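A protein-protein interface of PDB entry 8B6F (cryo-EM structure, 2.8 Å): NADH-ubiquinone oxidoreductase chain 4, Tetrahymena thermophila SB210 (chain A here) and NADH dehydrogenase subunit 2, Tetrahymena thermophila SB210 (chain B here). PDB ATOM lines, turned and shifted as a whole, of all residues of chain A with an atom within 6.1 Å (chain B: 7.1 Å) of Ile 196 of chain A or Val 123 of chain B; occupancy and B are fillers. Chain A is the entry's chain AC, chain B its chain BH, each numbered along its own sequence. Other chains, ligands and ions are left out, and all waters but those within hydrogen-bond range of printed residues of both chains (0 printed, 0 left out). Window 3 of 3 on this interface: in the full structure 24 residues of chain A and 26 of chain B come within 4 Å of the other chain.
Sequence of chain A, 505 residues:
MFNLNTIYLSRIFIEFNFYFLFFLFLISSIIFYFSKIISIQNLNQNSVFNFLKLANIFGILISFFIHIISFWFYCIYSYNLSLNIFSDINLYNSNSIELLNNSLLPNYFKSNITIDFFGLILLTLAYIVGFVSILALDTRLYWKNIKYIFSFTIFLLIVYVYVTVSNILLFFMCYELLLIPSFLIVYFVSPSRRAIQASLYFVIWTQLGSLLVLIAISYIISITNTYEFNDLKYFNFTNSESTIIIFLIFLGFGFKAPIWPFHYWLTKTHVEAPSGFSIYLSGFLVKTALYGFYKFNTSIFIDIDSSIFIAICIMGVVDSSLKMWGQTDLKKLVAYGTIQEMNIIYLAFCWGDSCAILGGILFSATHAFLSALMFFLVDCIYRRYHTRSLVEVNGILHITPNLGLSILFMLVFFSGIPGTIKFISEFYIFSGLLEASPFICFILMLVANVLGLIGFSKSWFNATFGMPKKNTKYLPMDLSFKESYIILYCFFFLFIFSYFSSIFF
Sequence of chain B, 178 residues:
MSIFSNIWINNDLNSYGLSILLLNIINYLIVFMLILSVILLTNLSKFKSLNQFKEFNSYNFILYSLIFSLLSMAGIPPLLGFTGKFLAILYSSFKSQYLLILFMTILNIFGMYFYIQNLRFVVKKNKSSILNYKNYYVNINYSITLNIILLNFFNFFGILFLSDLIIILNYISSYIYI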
ATOM      1  N   VAL A 186     -17.516  14.038 -12.361  1.00  0.00           N
ATOM      2  CA  VAL A 186     -18.687  14.545 -11.653  1.00  0.00           C
ATOM      3  C   VAL A 186     -19.468  15.499 -12.543  1.00  0.00           C
ATOM      4  O   VAL A 186     -20.704  15.536 -12.507  1.00  0.00           O
ATOM      5  CB  VAL A 186     -18.265  15.220 -10.334  1.00  0.00           C
ATOM      6  CG1 VAL A 186     -19.464  15.853  -9.642  1.00  0.00           C
ATOM      7  CG2 VAL A 186     -17.596  14.217  -9.415  1.00  0.00           C
ATOM      8  N   TYR A 187     -18.762  16.288 -13.354  1.00  0.00           N
ATOM      9  CA  TYR A 187     -19.425  17.324 -14.136  1.00  0.00           C
ATOM     10  C   TYR A 187     -20.196  16.737 -15.310  1.00  0.00           C
ATOM     11  O   TYR A 187     -21.326  17.157 -15.586  1.00  0.00           O
ATOM     12  CB  TYR A 187     -18.381  18.329 -14.623  1.00  0.00           C
ATOM     13  CG  TYR A 187     -18.938  19.548 -15.318  1.00  0.00           C
ATOM     14  CD1 TYR A 187     -19.387  20.643 -14.593  1.00  0.00           C
ATOM     15  CD2 TYR A 187     -18.984  19.615 -16.702  1.00  0.00           C
ATOM     16  CE1 TYR A 187     -19.883  21.764 -15.231  1.00  0.00           C
ATOM     17  CE2 TYR A 187     -19.477  20.728 -17.349  1.00  0.00           C
ATOM     18  CZ  TYR A 187     -19.924  21.800 -16.610  1.00  0.00           C
ATOM     19  OH  TYR A 187     -20.417  22.909 -17.254  1.00  0.00           O
ATOM     20  N   SER A 192     -27.884  13.735 -11.905  1.00  0.00           N
ATOM     21  CA  SER A 192     -28.647  14.774 -11.231  1.00  0.00           C
ATOM     22  C   SER A 192     -28.193  16.161 -11.672  1.00  0.00           C
ATOM     23  O   SER A 192     -27.027  16.387 -12.000  1.00  0.00           O
ATOM     24  CB  SER A 192     -28.503  14.637  -9.716  1.00  0.00           C
ATOM     25  OG  SER A 192     -29.258  15.626  -9.040  1.00  0.00           O
ATOM     26  N   ARG A 193     -29.142  17.101 -11.673  1.00  0.00           N
ATOM     27  CA  ARG A 193     -28.842  18.468 -12.085  1.00  0.00           C
ATOM     28  C   ARG A 193     -28.063  19.222 -11.018  1.00  0.00           C
ATOM     29  O   ARG A 193     -27.324  20.159 -11.340  1.00  0.00           O
ATOM     30  CB  ARG A 193     -30.135  19.211 -12.415  1.00  0.00           C
ATOM     31  CG  ARG A 193     -29.908  20.541 -13.105  1.00  0.00           C
ATOM     32  CD  ARG A 193     -31.221  21.199 -13.476  1.00  0.00           C
ATOM     33  NE  ARG A 193     -31.959  21.647 -12.301  1.00  0.00           N
ATOM     34  CZ  ARG A 193     -33.110  22.302 -12.347  1.00  0.00           C
ATOM     35  NH1 ARG A 193     -33.691  22.598 -13.498  1.00  0.00           N
ATOM     36  NH2 ARG A 193     -33.692  22.672 -11.210  1.00  0.00           N
ATOM     37  N   ARG A 194     -28.215  18.839  -9.752  1.00  0.00           N
ATOM     38  CA  ARG A 194     -27.464  19.474  -8.677  1.00  0.00           C
ATOM     39  C   ARG A 194     -25.986  19.125  -8.719  1.00  0.00           C
ATOM     40  O   ARG A 194     -25.198  19.746  -7.998  1.00  0.00           O
ATOM     41  CB  ARG A 194     -28.049  19.074  -7.324  1.00  0.00           C
ATOM     42  CG  ARG A 194     -29.537  19.340  -7.204  1.00  0.00           C
ATOM     43  CD  ARG A 194     -30.064  18.958  -5.833  1.00  0.00           C
ATOM     44  NE  ARG A 194     -31.500  19.184  -5.734  1.00  0.00           N
ATOM     45  CZ  ARG A 194     -32.060  20.341  -5.407  1.00  0.00           C
ATOM     46  NH1 ARG A 194     -31.331  21.411  -5.133  1.00  0.00           N
ATOM     47  NH2 ARG A 194     -33.386  20.430  -5.358  1.00  0.00           N
ATOM     48  N   ALA A 195     -25.597  18.143  -9.531  1.00  0.00           N
ATOM     49  CA  ALA A 195     -24.188  17.797  -9.657  1.00  0.00           C
ATOM     50  C   ALA A 195     -23.367  18.963 -10.186  1.00  0.00           C
ATOM     51  O   ALA A 195     -22.164  19.046  -9.917  1.00  0.00           O
ATOM     52  CB  ALA A 195     -24.039  16.599 -10.583  1.00  0.00           C
ATOM     53  N   ILE A 196     -23.990  19.862 -10.947  1.00  0.00           N
ATOM     54  CA  ILE A 196     -23.259  21.000 -11.498  1.00  0.00           C
ATOM     55  C   ILE A 196     -22.729  21.878 -10.372  1.00  0.00           C
ATOM     56  O   ILE A 196     -21.568  22.304 -10.386  1.00  0.00           O
ATOM     57  CB  ILE A 196     -24.153  21.796 -12.464  1.00  0.00           C
ATOM     58  CG1 ILE A 196     -24.764  20.875 -13.526  1.00  0.00           C
ATOM     59  CG2 ILE A 196     -23.356  22.909 -13.129  1.00  0.00           C
ATOM     60  CD1 ILE A 196     -23.757  20.038 -14.293  1.00  0.00           C
ATOM     61  N   GLN A 197     -23.573  22.165  -9.380  1.00  0.00           N
ATOM     62  CA  GLN A 197     -23.118  22.944  -8.234  1.00  0.00           C
ATOM     63  C   GLN A 197     -22.247  22.113  -7.302  1.00  0.00           C
ATOM     64  O   GLN A 197     -21.296  22.638  -6.713  1.00  0.00           O
ATOM     65  CB  GLN A 197     -24.317  23.504  -7.471  1.00  0.00           C
ATOM     66  CG  GLN A 197     -23.964  24.607  -6.488  1.00  0.00           C
ATOM     67  CD  GLN A 197     -23.544  25.885  -7.177  1.00  0.00           C
ATOM     68  OE1 GLN A 197     -23.639  26.005  -8.395  1.00  0.00           O
ATOM     69  NE2 GLN A 197     -23.075  26.851  -6.398  1.00  0.00           N
ATOM     70  N   ALA A 198     -22.547  20.821  -7.162  1.00  0.00           N
ATOM     71  CA  ALA A 198     -21.729  19.961  -6.313  1.00  0.00           C
ATOM     72  C   ALA A 198     -20.290  19.911  -6.806  1.00  0.00           C
ATOM     73  O   ALA A 198     -19.350  19.907  -6.004  1.00  0.00           O
ATOM     74  CB  ALA A 198     -22.325  18.556  -6.261  1.00  0.00           C
ATOM     75  N   SER A 199     -20.099  19.876  -8.125  1.00  0.00           N
ATOM     76  CA  SER A 199     -18.748  19.843  -8.676  1.00  0.00           C
ATOM     77  C   SER A 199     -17.980  21.111  -8.328  1.00  0.00           C
ATOM     78  O   SER A 199     -16.799  21.048  -7.968  1.00  0.00           O
ATOM     79  CB  SER A 199     -18.804  19.645 -10.190  1.00  0.00           C
ATOM     80  OG  SER A 199     -19.529  20.688 -10.815  1.00  0.00           O
ATOM     81  N   LEU A 200     -18.628  22.272  -8.428  1.00  0.00           N
ATOM     82  CA  LEU A 200     -17.954  23.517  -8.075  1.00  0.00           C
ATOM     83  C   LEU A 200     -17.591  23.543  -6.597  1.00  0.00           C
ATOM     84  O   LEU A 200     -16.494  23.977  -6.228  1.00  0.00           O
ATOM     85  CB  LEU A 200     -18.830  24.716  -8.435  1.00  0.00           C
ATOM     86  CG  LEU A 200     -19.332  24.793  -9.880  1.00  0.00           C
ATOM     87  CD1 LEU A 200     -19.723  26.220 -10.200  1.00  0.00           C
ATOM     88  CD2 LEU A 200     -18.314  24.278 -10.892  1.00  0.00           C
ATOM     89  N   TYR A 201     -18.500  23.091  -5.732  1.00  0.00           N
ATOM     90  CA  TYR A 201     -18.192  23.031  -4.308  1.00  0.00           C
ATOM     91  C   TYR A 201     -17.005  22.111  -4.058  1.00  0.00           C
ATOM     92  O   TYR A 201     -16.097  22.441  -3.289  1.00  0.00           O
ATOM     93  CB  TYR A 201     -19.412  22.553  -3.517  1.00  0.00           C
ATOM     94  CG  TYR A 201     -20.555  23.542  -3.448  1.00  0.00           C
ATOM     95  CD1 TYR A 201     -20.348  24.902  -3.638  1.00  0.00           C
ATOM     96  CD2 TYR A 201     -21.845  23.109  -3.180  1.00  0.00           C
ATOM     97  CE1 TYR A 201     -21.394  25.799  -3.569  1.00  0.00           C
ATOM     98  CE2 TYR A 201     -22.895  23.999  -3.109  1.00  0.00           C
ATOM     99  CZ  TYR A 201     -22.664  25.341  -3.305  1.00  0.00           C
ATOM    100  OH  TYR A 201     -23.711  26.228  -3.233  1.00  0.00           O
ATOM    101  N   GLU A 272     -24.857  14.193  -4.806  1.00  0.00           N
ATOM    102  CA  GLU A 272     -25.201  14.590  -6.164  1.00  0.00           C
ATOM    103  C   GLU A 272     -24.283  13.995  -7.230  1.00  0.00           C
ATOM    104  O   GLU A 272     -24.407  14.361  -8.402  1.00  0.00           O
ATOM    105  CB  GLU A 272     -25.186  16.116  -6.274  1.00  0.00           C
ATOM    106  CG  GLU A 272     -25.983  16.828  -5.189  1.00  0.00           C
ATOM    107  CD  GLU A 272     -27.450  16.446  -5.185  1.00  0.00           C
ATOM    108  OE1 GLU A 272     -27.908  15.818  -6.162  1.00  0.00           O
ATOM    109  OE2 GLU A 272     -28.147  16.773  -4.201  1.00  0.00           O
ATOM    110  N   ASN B  51     -24.113  34.516 -18.455  1.00  0.00           N
ATOM    111  CA  ASN B  51     -25.056  33.467 -18.812  1.00  0.00           C
ATOM    112  C   ASN B  51     -24.728  32.870 -20.172  1.00  0.00           C
ATOM    113  O   ASN B  51     -24.935  31.671 -20.390  1.00  0.00           O
ATOM    114  CB  ASN B  51     -26.471  34.041 -18.811  1.00  0.00           C
ATOM    115  CG  ASN B  51     -27.445  33.181 -19.570  1.00  0.00           C
ATOM    116  OD1 ASN B  51     -27.405  31.956 -19.485  1.00  0.00           O
ATOM    117  ND2 ASN B  51     -28.330  33.819 -20.327  1.00  0.00           N
ATOM    118  N   PHE B  53     -22.118  31.925 -21.398  1.00  0.00           N
ATOM    119  CA  PHE B  53     -21.113  30.869 -21.424  1.00  0.00           C
ATOM    120  C   PHE B  53     -21.707  29.560 -21.920  1.00  0.00           C
ATOM    121  O   PHE B  53     -20.985  28.710 -22.450  1.00  0.00           O
ATOM    122  CB  PHE B  53     -20.503  30.679 -20.036  1.00  0.00           C
ATOM    123  CG  PHE B  53     -19.214  31.416 -19.837  1.00  0.00           C
ATOM    124  CD1 PHE B  53     -18.025  30.891 -20.312  1.00  0.00           C
ATOM    125  CD2 PHE B  53     -19.188  32.628 -19.170  1.00  0.00           C
ATOM    126  CE1 PHE B  53     -16.835  31.564 -20.131  1.00  0.00           C
ATOM    127  CE2 PHE B  53     -17.999  33.306 -18.985  1.00  0.00           C
ATOM    128  CZ  PHE B  53     -16.822  32.772 -19.467  1.00  0.00           C
ATOM    129  N   LYS B  54     -23.019  29.379 -21.757  1.00  0.00           N
ATOM    130  CA  LYS B  54     -23.678  28.207 -22.318  1.00  0.00           C
ATOM    131  C   LYS B  54     -23.506  28.145 -23.827  1.00  0.00           C
ATOM    132  O   LYS B  54     -23.498  27.054 -24.407  1.00  0.00           O
ATOM    133  CB  LYS B  54     -25.163  28.216 -21.954  1.00  0.00           C
ATOM    134  CG  LYS B  54     -25.938  29.390 -22.530  1.00  0.00           C
ATOM    135  CD  LYS B  54     -27.383  29.371 -22.068  1.00  0.00           C
ATOM    136  CE  LYS B  54     -28.129  30.601 -22.547  1.00  0.00           C
ATOM    137  NZ  LYS B  54     -29.550  30.593 -22.107  1.00  0.00           N
ATOM    138  N   GLU B  55     -23.366  29.300 -24.482  1.00  0.00           N
ATOM    139  CA  GLU B  55     -23.171  29.312 -25.925  1.00  0.00           C
ATOM    140  C   GLU B  55     -21.903  28.583 -26.336  1.00  0.00           C
ATOM    141  O   GLU B  55     -21.812  28.118 -27.477  1.00  0.00           O
ATOM    142  CB  GLU B  55     -23.128  30.752 -26.436  1.00  0.00           C
ATOM    143  CG  GLU B  55     -24.399  31.537 -26.168  1.00  0.00           C
ATOM    144  CD  GLU B  55     -25.603  30.964 -26.885  1.00  0.00           C
ATOM    145  OE1 GLU B  55     -25.418  30.116 -27.781  1.00  0.00           O
ATOM    146  OE2 GLU B  55     -26.739  31.364 -26.555  1.00  0.00           O
ATOM    147  N   ASN B  57     -21.309  25.769 -25.345  1.00  0.00           N
ATOM    148  CA  ASN B  57     -21.708  24.370 -25.369  1.00  0.00           C
ATOM    149  C   ASN B  57     -21.919  23.948 -26.816  1.00  0.00           C
ATOM    150  O   ASN B  57     -23.053  23.793 -27.278  1.00  0.00           O
ATOM    151  CB  ASN B  57     -22.972  24.147 -24.541  1.00  0.00           C
ATOM    152  CG  ASN B  57     -23.240  22.682 -24.281  1.00  0.00           C
ATOM    153  OD1 ASN B  57     -22.958  21.830 -25.120  1.00  0.00           O
ATOM    154  ND2 ASN B  57     -23.778  22.379 -23.108  1.00  0.00           N
ATOM    155  N   LEU B  63     -15.986  23.009 -26.704  1.00  0.00           N
ATOM    156  CA  LEU B  63     -16.456  22.877 -25.330  1.00  0.00           C
ATOM    157  C   LEU B  63     -15.299  22.618 -24.376  1.00  0.00           C
ATOM    158  O   LEU B  63     -15.130  23.328 -23.379  1.00  0.00           O
ATOM    159  CB  LEU B  63     -17.487  21.751 -25.241  1.00  0.00           C
ATOM    160  CG  LEU B  63     -17.983  21.385 -23.840  1.00  0.00           C
ATOM    161  CD1 LEU B  63     -18.579  22.589 -23.132  1.00  0.00           C
ATOM    162  CD2 LEU B  63     -19.000  20.262 -23.926  1.00  0.00           C
ATOM    163  N   ASN B 118     -18.249  30.106 -13.798  1.00  0.00           N
ATOM    164  CA  ASN B 118     -18.740  30.122 -15.170  1.00  0.00           C
ATOM    165  C   ASN B 118     -18.936  28.724 -15.736  1.00  0.00           C
ATOM    166  O   ASN B 118     -19.716  28.557 -16.678  1.00  0.00           O
ATOM    167  CB  ASN B 118     -17.776  30.906 -16.056  1.00  0.00           C
ATOM    168  CG  ASN B 118     -17.643  32.348 -15.628  1.00  0.00           C
ATOM    169  OD1 ASN B 118     -18.607  32.964 -15.179  1.00  0.00           O
ATOM    170  ND2 ASN B 118     -16.443  32.893 -15.757  1.00  0.00           N
ATOM    171  N   LEU B 119     -18.256  27.718 -15.186  1.00  0.00           N
ATOM    172  CA  LEU B 119     -18.493  26.346 -15.621  1.00  0.00           C
ATOM    173  C   LEU B 119     -19.932  25.929 -15.359  1.00  0.00           C
ATOM    174  O   LEU B 119     -20.477  25.088 -16.081  1.00  0.00           O
ATOM    175  CB  LEU B 119     -17.520  25.400 -14.921  1.00  0.00           C
ATOM    176  CG  LEU B 119     -16.038  25.685 -15.180  1.00  0.00           C
ATOM    177  CD1 LEU B 119     -15.163  24.821 -14.297  1.00  0.00           C
ATOM    178  CD2 LEU B 119     -15.690  25.462 -16.643  1.00  0.00           C
ATOM    179  N   ARG B 120     -20.559  26.503 -14.331  1.00  0.00           N
ATOM    180  CA  ARG B 120     -21.975  26.253 -14.091  1.00  0.00           C
ATOM    181  C   ARG B 120     -22.822  26.766 -15.246  1.00  0.00           C
ATOM    182  O   ARG B 120     -23.761  26.093 -15.686  1.00  0.00           O
ATOM    183  CB  ARG B 120     -22.403  26.912 -12.780  1.00  0.00           C
ATOM    184  CG  ARG B 120     -23.834  26.626 -12.372  1.00  0.00           C
ATOM    185  CD  ARG B 120     -24.162  27.317 -11.061  1.00  0.00           C
ATOM    186  NE  ARG B 120     -25.369  26.780 -10.443  1.00  0.00           N
ATOM    187  CZ  ARG B 120     -26.593  27.255 -10.633  1.00  0.00           C
ATOM    188  NH1 ARG B 120     -26.820  28.289 -11.423  1.00  0.00           N
ATOM    189  NH2 ARG B 120     -27.616  26.676 -10.013  1.00  0.00           N
ATOM    190  N   PHE B 121     -22.504  27.959 -15.752  1.00  0.00           N
ATOM    191  CA  PHE B 121     -23.270  28.522 -16.857  1.00  0.00           C
ATOM    192  C   PHE B 121     -22.976  27.807 -18.168  1.00  0.00           C
ATOM    193  O   PHE B 121     -23.816  27.810 -19.074  1.00  0.00           O
ATOM    194  CB  PHE B 121     -22.963  30.013 -16.993  1.00  0.00           C
ATOM    195  CG  PHE B 121     -23.023  30.764 -15.693  1.00  0.00           C
ATOM    196  CD1 PHE B 121     -23.943  30.420 -14.718  1.00  0.00           C
ATOM    197  CD2 PHE B 121     -22.151  31.810 -15.446  1.00  0.00           C
ATOM    198  CE1 PHE B 121     -23.994  31.108 -13.523  1.00  0.00           C
ATOM    199  CE2 PHE B 121     -22.198  32.502 -14.252  1.00  0.00           C
ATOM    200  CZ  PHE B 121     -23.121  32.150 -13.291  1.00  0.00           C
ATOM    201  N   VAL B 122     -21.797  27.195 -18.294  1.00  0.00           N
ATOM    202  CA  VAL B 122     -21.442  26.503 -19.530  1.00  0.00           C
ATOM    203  C   VAL B 122     -22.465  25.427 -19.866  1.00  0.00           C
ATOM    204  O   VAL B 122     -22.662  25.094 -21.040  1.00  0.00           O
ATOM    205  CB  VAL B 122     -20.019  25.916 -19.422  1.00  0.00           C
ATOM    206  CG1 VAL B 122     -19.767  24.879 -20.511  1.00  0.00           C
ATOM    207  CG2 VAL B 122     -18.981  27.022 -19.503  1.00  0.00           C
ATOM    208  N   VAL B 123     -23.124  24.858 -18.856  1.00  0.00           N
ATOM    209  CA  VAL B 123     -24.125  23.831 -19.116  1.00  0.00           C
ATOM    210  C   VAL B 123     -25.282  24.442 -19.888  1.00  0.00           C
ATOM    211  O   VAL B 123     -25.796  25.509 -19.532  1.00  0.00           O
ATOM    212  CB  VAL B 123     -24.599  23.200 -17.799  1.00  0.00           C
ATOM    213  CG1 VAL B 123     -25.694  22.176 -18.056  1.00  0.00           C
ATOM    214  CG2 VAL B 123     -23.435  22.564 -17.061  1.00  0.00           C
ATOM    215  N   LYS B 124     -25.705  23.758 -20.949  1.00  0.00           N
ATOM    216  CA  LYS B 124     -26.761  24.242 -21.825  1.00  0.00           C
ATOM    217  C   LYS B 124     -27.767  23.130 -22.074  1.00  0.00           C
ATOM    218  O   LYS B 124     -27.411  21.951 -22.134  1.00  0.00           O
ATOM    219  CB  LYS B 124     -26.194  24.738 -23.160  1.00  0.00           C
ATOM    220  CG  LYS B 124     -27.209  25.455 -24.030  1.00  0.00           C
ATOM    221  CD  LYS B 124     -26.567  26.012 -25.288  1.00  0.00           C
ATOM    222  CE  LYS B 124     -27.619  26.517 -26.264  1.00  0.00           C
ATOM    223  NZ  LYS B 124     -28.478  27.579 -25.680  1.00  0.00           N
ATOM    224  N   LYS B 125     -29.033  23.523 -22.232  1.00  0.00           N
ATOM    225  CA  LYS B 125     -30.088  22.542 -22.458  1.00  0.00           C
ATOM    226  C   LYS B 125     -29.861  21.777 -23.755  1.00  0.00           C
ATOM    227  O   LYS B 125     -30.040  20.555 -23.804  1.00  0.00           O
ATOM    228  CB  LYS B 125     -31.446  23.241 -22.474  1.00  0.00           C
ATOM    229  CG  LYS B 125     -32.624  22.308 -22.699  1.00  0.00           C
ATOM    230  CD  LYS B 125     -33.949  23.058 -22.661  1.00  0.00           C
ATOM    231  CE  LYS B 125     -34.079  24.028 -23.828  1.00  0.00           C
ATOM    232  NZ  LYS B 125     -35.407  24.705 -23.839  1.00  0.00           N
ATOM    233  N   ASN B 126     -29.475  22.480 -24.818  1.00  0.00           N
ATOM    234  CA  ASN B 126     -29.169  21.853 -26.097  1.00  0.00           C
ATOM    235  C   ASN B 126     -27.793  22.289 -26.577  1.00  0.00           C
ATOM    236  O   ASN B 126     -27.054  22.949 -25.841  1.00  0.00           O
ATOM    237  CB  ASN B 126     -30.232  22.209 -27.137  1.00  0.00           C
ATOM    238  CG  ASN B 126     -31.616  21.737 -26.737  1.00  0.00           C
ATOM    239  OD1 ASN B 126     -32.535  22.540 -26.574  1.00  0.00           O
ATOM    240  ND2 ASN B 126     -31.771  20.427 -26.579  1.00  0.00           N
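Ile 196 of chain A touches just these residues of chain B: Arg 120 (3.7 Å) and Val 123 (3.8 Å). Val 123 of chain B touches just these residues of chain A: Tyr 187 (3.0 Å) and Ile 196 (3.8 Å). Of the printed residues of chain B, Leu 200 of chain A touches Arg 120. Printed residues of chain A within 4 Å of Leu 119 of chain B: Tyr 187 (2.5 Å). Of the printed residues of chain A, Val 122 of chain B touches Tyr 187. Of the printed residues of chain B, Gln 197 of chain A touches Arg 120. Of the printed residues of chain B, Tyr 187 of chain A touches Leu 119 (2.5 Å), Val 122 (3.7 Å) and Val 123 (3.0 Å). Lys 54 of chain B touches none of the printed residues of chain A. The nearest printed residue of chain A that does not touch Val 123 of chain B is Arg 193 of chain A (6.7 Å). The nearest printed residue of chain B that does not touch Leu 200 of chain A is Leu 119 of chain B (4.3 Å).
NE2 of Gln 197 of chain A lies within hydrogen-bond range of OH of Tyr 201 of chain A (3.3 Å). O of Ile 196 of chain A lies within hydrogen-bond range of OG of Ser 199 of chain A.
Printed residues of chain B that touch a printed residue of chain A: Leu 119, Arg 120, Val 122 and Val 123. Along chain B the printed residues that touch a printed residue of chain A span positions 119 to 123. Of the 13 printed residues of chain A, 4 touch a printed residue of chain B. Hydrophobic or aromatic side chains of chain A within 4 Å of the printed part of chain B: Tyr 187, Ile 196 and Leu 200. Along chain A the printed residues that touch a printed residue of chain B span positions 187 to 200. Among the printed residues, 7 pairs touch across the chains. Among the printed residues, no Asp or Glu carboxylate lies within 4 Å of a Lys or Arg side-chain nitrogen of the other chain.
Among the printed residues, merely in contact across the chains: Tyr 187 of chain A with Val 122 of chain B (3.7 Å), Tyr 187 of chain A with Val 123 of chain B (3.0 Å), Ile 196 of chain A with Arg 120 of chain B (3.7 Å), Ile 196 of chain A with Val 123 of chain B (3.8 Å) and Leu 200 of chain A with Arg 120 of chain B (3.8 Å).
The side-chain amide oxygen of Gln 197 of chain A lies within hydrogen-bond range of the guanidinium group of Arg 120 of chain B, 2.8 Å away. OH of Tyr 187 of chain A lies within hydrogen-bond range of O of Leu 119 of chain B.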
